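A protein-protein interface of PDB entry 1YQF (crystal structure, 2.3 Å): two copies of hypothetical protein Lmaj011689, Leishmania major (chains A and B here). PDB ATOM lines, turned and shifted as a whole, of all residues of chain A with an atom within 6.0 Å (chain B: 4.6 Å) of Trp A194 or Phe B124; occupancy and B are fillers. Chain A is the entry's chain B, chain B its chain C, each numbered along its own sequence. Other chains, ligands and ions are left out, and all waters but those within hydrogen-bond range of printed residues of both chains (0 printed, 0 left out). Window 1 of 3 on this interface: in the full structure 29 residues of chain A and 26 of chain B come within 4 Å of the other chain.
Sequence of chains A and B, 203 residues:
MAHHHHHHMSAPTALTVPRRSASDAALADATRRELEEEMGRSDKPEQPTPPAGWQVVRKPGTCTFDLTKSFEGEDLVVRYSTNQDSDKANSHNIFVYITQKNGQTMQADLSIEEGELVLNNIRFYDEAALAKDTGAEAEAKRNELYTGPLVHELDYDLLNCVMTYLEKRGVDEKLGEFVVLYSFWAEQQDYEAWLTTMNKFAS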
ATOM      1  N   GLN A 189      38.520  28.646  -4.868  1.00  0.00           N
ATOM      2  CA  GLN A 189      38.494  27.213  -5.175  1.00  0.00           C
ATOM      3  C   GLN A 189      37.109  26.608  -4.978  1.00  0.00           C
ATOM      4  O   GLN A 189      36.624  25.870  -5.830  1.00  0.00           O
ATOM      5  CB  GLN A 189      39.491  26.448  -4.295  1.00  0.00           C
ATOM      6  CG  GLN A 189      40.950  26.801  -4.523  1.00  0.00           C
ATOM      7  CD  GLN A 189      41.403  26.549  -5.948  1.00  0.00           C
ATOM      8  OE1 GLN A 189      41.353  25.415  -6.431  1.00  0.00           O
ATOM      9  NE2 GLN A 189      41.845  27.602  -6.625  1.00  0.00           N
ATOM     10  N   ASP A 190      36.487  26.914  -3.843  1.00  0.00           N
ATOM     11  CA  ASP A 190      35.145  26.427  -3.538  1.00  0.00           C
ATOM     12  C   ASP A 190      34.108  26.980  -4.509  1.00  0.00           C
ATOM     13  O   ASP A 190      33.164  26.279  -4.856  1.00  0.00           O
ATOM     14  CB  ASP A 190      34.744  26.791  -2.106  1.00  0.00           C
ATOM     15  CG  ASP A 190      35.563  26.049  -1.058  1.00  0.00           C
ATOM     16  OD1 ASP A 190      36.148  24.988  -1.376  1.00  0.00           O
ATOM     17  OD2 ASP A 190      35.673  26.461   0.120  1.00  0.00           O
ATOM     18  N   TYR A 191      34.286  28.229  -4.940  1.00  0.00           N
ATOM     19  CA  TYR A 191      33.381  28.851  -5.909  1.00  0.00           C
ATOM     20  C   TYR A 191      33.465  28.141  -7.259  1.00  0.00           C
ATOM     21  O   TYR A 191      32.455  27.962  -7.930  1.00  0.00           O
ATOM     22  CB  TYR A 191      33.695  30.340  -6.084  1.00  0.00           C
ATOM     23  CG  TYR A 191      32.807  31.033  -7.108  1.00  0.00           C
ATOM     24  CD1 TYR A 191      31.422  31.031  -6.971  1.00  0.00           C
ATOM     25  CD2 TYR A 191      33.356  31.688  -8.212  1.00  0.00           C
ATOM     26  CE1 TYR A 191      30.604  31.658  -7.905  1.00  0.00           C
ATOM     27  CE2 TYR A 191      32.548  32.319  -9.150  1.00  0.00           C
ATOM     28  CZ  TYR A 191      31.171  32.301  -8.993  1.00  0.00           C
ATOM     29  OH  TYR A 191      30.363  32.925  -9.919  1.00  0.00           O
ATOM     30  N   GLU A 192      34.672  27.733  -7.643  1.00  0.00           N
ATOM     31  CA  GLU A 192      34.880  27.004  -8.896  1.00  0.00           C
ATOM     32  C   GLU A 192      34.242  25.617  -8.844  1.00  0.00           C
ATOM     33  O   GLU A 192      33.629  25.179  -9.812  1.00  0.00           O
ATOM     34  CB  GLU A 192      36.371  26.861  -9.202  1.00  0.00           C
ATOM     35  CG  GLU A 192      36.984  28.057  -9.908  1.00  0.00           C
ATOM     36  CD  GLU A 192      38.499  27.990  -9.946  1.00  0.00           C
ATOM     37  OE1 GLU A 192      39.046  26.875 -10.113  1.00  0.00           O
ATOM     38  OE2 GLU A 192      39.143  29.050  -9.804  1.00  0.00           O
ATOM     39  N   ALA A 193      34.397  24.936  -7.711  1.00  0.00           N
ATOM     40  CA  ALA A 193      33.788  23.623  -7.491  1.00  0.00           C
ATOM     41  C   ALA A 193      32.267  23.740  -7.378  1.00  0.00           C
ATOM     42  O   ALA A 193      31.537  22.799  -7.684  1.00  0.00           O
ATOM     43  CB  ALA A 193      34.362  22.979  -6.221  1.00  0.00           C
ATOM     44  N   TRP A 194      31.803  24.906  -6.936  1.00  0.00           N
ATOM     45  CA  TRP A 194      30.380  25.206  -6.823  1.00  0.00           C
ATOM     46  C   TRP A 194      29.728  25.315  -8.201  1.00  0.00           C
ATOM     47  O   TRP A 194      28.625  24.816  -8.407  1.00  0.00           O
ATOM     48  CB  TRP A 194      30.205  26.511  -6.047  1.00  0.00           C
ATOM     49  CG  TRP A 194      28.800  26.942  -5.803  1.00  0.00           C
ATOM     50  CD1 TRP A 194      27.972  26.521  -4.804  1.00  0.00           C
ATOM     51  CD2 TRP A 194      28.070  27.922  -6.543  1.00  0.00           C
ATOM     52  NE1 TRP A 194      26.763  27.168  -4.888  1.00  0.00           N
ATOM     53  CE2 TRP A 194      26.795  28.035  -5.949  1.00  0.00           C
ATOM     54  CE3 TRP A 194      28.362  28.718  -7.661  1.00  0.00           C
ATOM     55  CZ2 TRP A 194      25.815  28.907  -6.432  1.00  0.00           C
ATOM     56  CZ3 TRP A 194      27.383  29.582  -8.144  1.00  0.00           C
ATOM     57  CH2 TRP A 194      26.127  29.670  -7.526  1.00  0.00           C
ATOM     58  N   LEU A 195      30.420  25.970  -9.134  1.00  0.00           N
ATOM     59  CA  LEU A 195      29.949  26.120 -10.512  1.00  0.00           C
ATOM     60  C   LEU A 195      30.027  24.789 -11.245  1.00  0.00           C
ATOM     61  O   LEU A 195      29.186  24.484 -12.090  1.00  0.00           O
ATOM     62  CB  LEU A 195      30.799  27.144 -11.268  1.00  0.00           C
ATOM     63  CG  LEU A 195      30.668  28.618 -10.878  1.00  0.00           C
ATOM     64  CD1 LEU A 195      31.854  29.396 -11.410  1.00  0.00           C
ATOM     65  CD2 LEU A 195      29.368  29.213 -11.405  1.00  0.00           C
ATOM     66  N   THR A 196      31.055  24.009 -10.933  1.00  0.00           N
ATOM     67  CA  THR A 196      31.219  22.688 -11.513  1.00  0.00           C
ATOM     68  C   THR A 196      30.076  21.801 -11.046  1.00  0.00           C
ATOM     69  O   THR A 196      29.445  21.110 -11.852  1.00  0.00           O
ATOM     70  CB  THR A 196      32.573  22.086 -11.101  1.00  0.00           C
ATOM     71  OG1 THR A 196      33.633  22.938 -11.554  1.00  0.00           O
ATOM     72  CG2 THR A 196      32.829  20.757 -11.817  1.00  0.00           C
ATOM     73  N   THR A 197      29.802  21.846  -9.745  1.00  0.00           N
ATOM     74  CA  THR A 197      28.705  21.087  -9.165  1.00  0.00           C
ATOM     75  C   THR A 197      27.377  21.508  -9.779  1.00  0.00           C
ATOM     76  O   THR A 197      26.602  20.657 -10.205  1.00  0.00           O
ATOM     77  CB  THR A 197      28.666  21.260  -7.641  1.00  0.00           C
ATOM     78  OG1 THR A 197      29.818  20.642  -7.048  1.00  0.00           O
ATOM     79  CG2 THR A 197      27.469  20.520  -7.031  1.00  0.00           C
ATOM     80  N   MET A 198      27.117  22.814  -9.823  1.00  0.00           N
ATOM     81  CA  MET A 198      25.857  23.322 -10.370  1.00  0.00           C
ATOM     82  C   MET A 198      25.713  22.983 -11.852  1.00  0.00           C
ATOM     83  O   MET A 198      24.610  22.706 -12.325  1.00  0.00           O
ATOM     84  CB  MET A 198      25.727  24.835 -10.185  1.00  0.00           C
ATOM     85  CG  MET A 198      24.413  25.379 -10.749  1.00  0.00           C
ATOM     86  SD  MET A 198      24.045  27.065 -10.307  1.00  0.00           S
ATOM     87  CE  MET A 198      23.485  26.818  -8.631  1.00  0.00           C
ATOM     88  N   ASN A 199      26.826  23.018 -12.579  1.00  0.00           N
ATOM     89  CA  ASN A 199      26.832  22.659 -13.995  1.00  0.00           C
ATOM     90  C   ASN A 199      26.459  21.190 -14.158  1.00  0.00           C
ATOM     91  O   ASN A 199      25.513  20.856 -14.870  1.00  0.00           O
ATOM     92  CB  ASN A 199      28.203  22.914 -14.627  1.00  0.00           C
ATOM     93  CG  ASN A 199      28.254  22.487 -16.087  1.00  0.00           C
ATOM     94  OD1 ASN A 199      27.829  23.226 -16.977  1.00  0.00           O
ATOM     95  ND2 ASN A 199      28.757  21.284 -16.334  1.00  0.00           N
ATOM     96  N   PHE A 201      24.910  19.512 -12.175  1.00  0.00           N
ATOM     97  CA  PHE A 201      23.530  19.434 -11.698  1.00  0.00           C
ATOM     98  C   PHE A 201      22.499  19.736 -12.785  1.00  0.00           C
ATOM     99  O   PHE A 201      21.437  19.119 -12.821  1.00  0.00           O
ATOM    100  CB  PHE A 201      23.329  20.404 -10.527  1.00  0.00           C
ATOM    101  CG  PHE A 201      22.394  19.899  -9.475  1.00  0.00           C
ATOM    102  CD1 PHE A 201      22.862  19.098  -8.442  1.00  0.00           C
ATOM    103  CD2 PHE A 201      21.048  20.228  -9.510  1.00  0.00           C
ATOM    104  CE1 PHE A 201      22.002  18.633  -7.460  1.00  0.00           C
ATOM    105  CE2 PHE A 201      20.180  19.765  -8.529  1.00  0.00           C
ATOM    106  CZ  PHE A 201      20.658  18.966  -7.505  1.00  0.00           C
ATOM    107  N   THR B 105      22.323  16.987  -3.470  1.00  0.00           N
ATOM    108  CA  THR B 105      21.209  17.887  -3.180  1.00  0.00           C
ATOM    109  C   THR B 105      21.580  19.361  -3.300  1.00  0.00           C
ATOM    110  O   THR B 105      22.596  19.795  -2.770  1.00  0.00           O
ATOM    111  CB  THR B 105      20.682  17.612  -1.766  1.00  0.00           C
ATOM    112  OG1 THR B 105      20.123  16.292  -1.709  1.00  0.00           O
ATOM    113  CG2 THR B 105      19.510  18.542  -1.433  1.00  0.00           C
ATOM    114  N   MET B 106      20.737  20.127  -3.990  1.00  0.00           N
ATOM    115  CA  MET B 106      20.848  21.583  -4.017  1.00  0.00           C
ATOM    116  C   MET B 106      19.862  22.196  -3.028  1.00  0.00           C
ATOM    117  O   MET B 106      18.702  21.799  -2.974  1.00  0.00           O
ATOM    118  CB  MET B 106      20.550  22.129  -5.414  1.00  0.00           C
ATOM    119  CG  MET B 106      20.836  23.630  -5.543  1.00  0.00           C
ATOM    120  SD  MET B 106      20.023  24.420  -6.934  1.00  0.00           S
ATOM    121  CE  MET B 106      20.956  23.766  -8.272  1.00  0.00           C
ATOM    122  N   ILE B 122      22.543  29.651  -2.155  1.00  0.00           N
ATOM    123  CA  ILE B 122      22.552  28.410  -2.929  1.00  0.00           C
ATOM    124  C   ILE B 122      23.755  27.577  -2.490  1.00  0.00           C
ATOM    125  O   ILE B 122      24.891  28.021  -2.626  1.00  0.00           O
ATOM    126  CB  ILE B 122      22.687  28.698  -4.436  1.00  0.00           C
ATOM    127  CG1 ILE B 122      21.567  29.604  -4.948  1.00  0.00           C
ATOM    128  CG2 ILE B 122      22.695  27.390  -5.228  1.00  0.00           C
ATOM    129  CD1 ILE B 122      21.878  30.208  -6.308  1.00  0.00           C
ATOM    130  N   ARG B 123      23.507  26.371  -1.983  1.00  0.00           N
ATOM    131  CA  ARG B 123      24.577  25.458  -1.577  1.00  0.00           C
ATOM    132  C   ARG B 123      24.271  24.011  -1.949  1.00  0.00           C
ATOM    133  O   ARG B 123      23.138  23.674  -2.281  1.00  0.00           O
ATOM    134  CB  ARG B 123      24.818  25.559  -0.073  1.00  0.00           C
ATOM    135  CG  ARG B 123      23.596  25.280   0.777  1.00  0.00           C
ATOM    136  CD  ARG B 123      23.803  25.575   2.241  1.00  0.00           C
ATOM    137  NE  ARG B 123      24.897  24.771   2.776  1.00  0.00           N
ATOM    138  CZ  ARG B 123      25.302  24.786   4.035  1.00  0.00           C
ATOM    139  NH1 ARG B 123      24.707  25.569   4.927  1.00  0.00           N
ATOM    140  NH2 ARG B 123      26.300  24.004   4.414  1.00  0.00           N
ATOM    141  N   PHE B 124      25.289  23.159  -1.865  1.00  0.00           N
ATOM    142  CA  PHE B 124      25.175  21.761  -2.265  1.00  0.00           C
ATOM    143  C   PHE B 124      25.651  20.812  -1.168  1.00  0.00           C
ATOM    144  O   PHE B 124      26.578  21.128  -0.421  1.00  0.00           O
ATOM    145  CB  PHE B 124      25.992  21.511  -3.529  1.00  0.00           C
ATOM    146  CG  PHE B 124      25.440  22.181  -4.750  1.00  0.00           C
ATOM    147  CD1 PHE B 124      24.418  21.590  -5.476  1.00  0.00           C
ATOM    148  CD2 PHE B 124      25.950  23.401  -5.180  1.00  0.00           C
ATOM    149  CE1 PHE B 124      23.910  22.204  -6.613  1.00  0.00           C
ATOM    150  CE2 PHE B 124      25.448  24.014  -6.306  1.00  0.00           C
ATOM    151  CZ  PHE B 124      24.426  23.415  -7.026  1.00  0.00           C
ATOM    152  N   TYR B 125      25.004  19.650  -1.091  1.00  0.00           N
ATOM    153  CA  TYR B 125      25.358  18.583  -0.154  1.00  0.00           C
ATOM    154  C   TYR B 125      25.470  17.258  -0.904  1.00  0.00           C
ATOM    155  O   TYR B 125      24.748  17.023  -1.866  1.00  0.00           O
ATOM    156  CB  TYR B 125      24.291  18.416   0.929  1.00  0.00           C
ATOM    157  CG  TYR B 125      23.942  19.651   1.720  1.00  0.00           C
ATOM    158  CD1 TYR B 125      24.653  19.995   2.865  1.00  0.00           C
ATOM    159  CD2 TYR B 125      22.870  20.456   1.346  1.00  0.00           C
ATOM    160  CE1 TYR B 125      24.316  21.122   3.607  1.00  0.00           C
ATOM    161  CE2 TYR B 125      22.524  21.580   2.079  1.00  0.00           C
ATOM    162  CZ  TYR B 125      23.249  21.912   3.208  1.00  0.00           C
ATOM    163  OH  TYR B 125      22.900  23.032   3.938  1.00  0.00           O
ATOM    164  N   ASP B 126      26.357  16.384  -0.439  1.00  0.00           N
ATOM    165  CA  ASP B 126      26.542  15.066  -1.051  1.00  0.00           C
ATOM    166  C   ASP B 126      25.339  14.155  -0.803  1.00  0.00           C
ATOM    167  O   ASP B 126      24.933  13.402  -1.688  1.00  0.00           O
ATOM    168  CB  ASP B 126      27.803  14.383  -0.503  1.00  0.00           C
ATOM    169  CG  ASP B 126      29.081  14.915  -1.124  1.00  0.00           C
ATOM    170  OD1 ASP B 126      29.113  15.603  -2.173  1.00  0.00           O
ATOM    171  OD2 ASP B 126      30.161  14.641  -0.561  1.00  0.00           O
ATOM    172  N   TYR B 146      30.900  24.422   3.032  1.00  0.00           N
ATOM    173  CA  TYR B 146      30.875  25.610   2.189  1.00  0.00           C
ATOM    174  C   TYR B 146      29.430  26.017   1.889  1.00  0.00           C
ATOM    175  O   TYR B 146      28.698  25.284   1.236  1.00  0.00           O
ATOM    176  CB  TYR B 146      31.631  25.334   0.884  1.00  0.00           C
ATOM    177  CG  TYR B 146      31.568  26.455  -0.129  1.00  0.00           C
ATOM    178  CD1 TYR B 146      32.044  27.725   0.177  1.00  0.00           C
ATOM    179  CD2 TYR B 146      31.033  26.243  -1.394  1.00  0.00           C
ATOM    180  CE1 TYR B 146      31.991  28.755  -0.753  1.00  0.00           C
ATOM    181  CE2 TYR B 146      30.975  27.265  -2.329  1.00  0.00           C
ATOM    182  CZ  TYR B 146      31.454  28.517  -2.005  1.00  0.00           C
ATOM    183  OH  TYR B 146      31.396  29.536  -2.932  1.00  0.00           O
ATOM    184  N   GLY B 148      28.313  28.301  -0.066  1.00  0.00           N
ATOM    185  CA  GLY B 148      28.122  28.882  -1.384  1.00  0.00           C
ATOM    186  C   GLY B 148      28.579  30.327  -1.413  1.00  0.00           C
ATOM    187  O   GLY B 148      28.892  30.895  -0.372  1.00  0.00           O
ATOM    188  N   PRO B 149      28.623  30.930  -2.596  1.00  0.00           N
ATOM    189  CA  PRO B 149      29.052  32.326  -2.721  1.00  0.00           C
ATOM    190  C   PRO B 149      27.974  33.289  -2.252  1.00  0.00           C
ATOM    191  O   PRO B 149      26.829  32.884  -2.022  1.00  0.00           O
ATOM    192  CB  PRO B 149      29.276  32.481  -4.225  1.00  0.00           C
ATOM    193  CG  PRO B 149      28.276  31.552  -4.819  1.00  0.00           C
ATOM    194  CD  PRO B 149      28.259  30.352  -3.901  1.00  0.00           C
ATOM    195  N   LEU B 154      26.383  37.952  -7.659  1.00  0.00           N
ATOM    196  CA  LEU B 154      26.478  37.124  -8.856  1.00  0.00           C
ATOM    197  C   LEU B 154      25.889  37.841 -10.064  1.00  0.00           C
ATOM    198  O   LEU B 154      24.999  38.682  -9.925  1.00  0.00           O
ATOM    199  CB  LEU B 154      25.766  35.779  -8.646  1.00  0.00           C
ATOM    200  CG  LEU B 154      26.377  34.847  -7.591  1.00  0.00           C
ATOM    201  CD1 LEU B 154      25.513  33.609  -7.388  1.00  0.00           C
ATOM    202  CD2 LEU B 154      27.799  34.446  -7.972  1.00  0.00           C
ATOM    203  N   LEU B 158      23.569  34.420 -14.712  1.00  0.00           N
ATOM    204  CA  LEU B 158      23.669  33.190 -13.936  1.00  0.00           C
ATOM    205  C   LEU B 158      22.510  33.067 -12.956  1.00  0.00           C
ATOM    206  O   LEU B 158      21.853  32.034 -12.890  1.00  0.00           O
ATOM    207  CB  LEU B 158      24.998  33.127 -13.180  1.00  0.00           C
ATOM    208  CG  LEU B 158      25.200  31.892 -12.288  1.00  0.00           C
ATOM    209  CD1 LEU B 158      25.026  30.590 -13.075  1.00  0.00           C
ATOM    210  CD2 LEU B 158      26.559  31.935 -11.635  1.00  0.00           C
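The indole nitrogen of Trp A194 sits at hydrogen-bond distance from the backbone carbonyl oxygen of Ile B122 (3.1 Å).
The backbone carbonyl oxygen (O) of Ala A193 is in hydrogen-bond range of the side-chain hydroxyl (OG1) of Thr A197, at 2.8 Å.
Among the printed residues, merely in contact across the chains: Asp A190 with Tyr B146, Tyr A191 with Tyr B146, Tyr A191 with Pro B149, Tyr A191 with Leu B154, Trp A194 with Phe B124, Trp A194 with Tyr B146, Trp A194 with Pro B149, Trp A194 with Leu B154, Leu A195 with Leu B158, Thr A197 with Phe B124, Met A198 with Met B106, Met A198 with Ile B122, Met A198 with Phe B124, Phe A201 with Met B106 and Phe A201 with Phe B124.
Printed residues of chain B within 4 Å of Trp A194: Ile B122 (3.1 Å), Phe B124 (3.7 Å), Tyr B146 (3.9 Å), Pro B149 (3.4 Å) and Leu B154 (3.99 Å).
Of the printed residues of chain B, Thr A197 touches Phe B124 (3.5 Å).
Phe B124 touches four residues of chain A.
Of the printed residues of chain A, Tyr B146 touches Asp A190, Tyr A191 and Trp A194.
Printed residues of chain A within 4 Å of Leu B154: Tyr A191 (3.6 Å) and Trp A194 (3.99 Å).
The nearest printed residue of chain A that does not touch Leu B158 is Tyr A191 (4.3 Å).
Hydrophobic or aromatic side chains of chain B within 4 Å of the printed part of chain A: Met B106, Ile B122, Phe B124, Tyr B146, Pro B149, Leu B154 and Leu B158.
Among the printed residues, 16 pairs touch across the chains.
Among the printed residues, no Asp or Glu carboxylate lies within 4 Å of a Lys or Arg side-chain nitrogen of the other chain.
No position is printed for both chains.
Of the 16 pairs that touch across the chains among the printed residues, none has its exchanged pair printed and touching as well.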
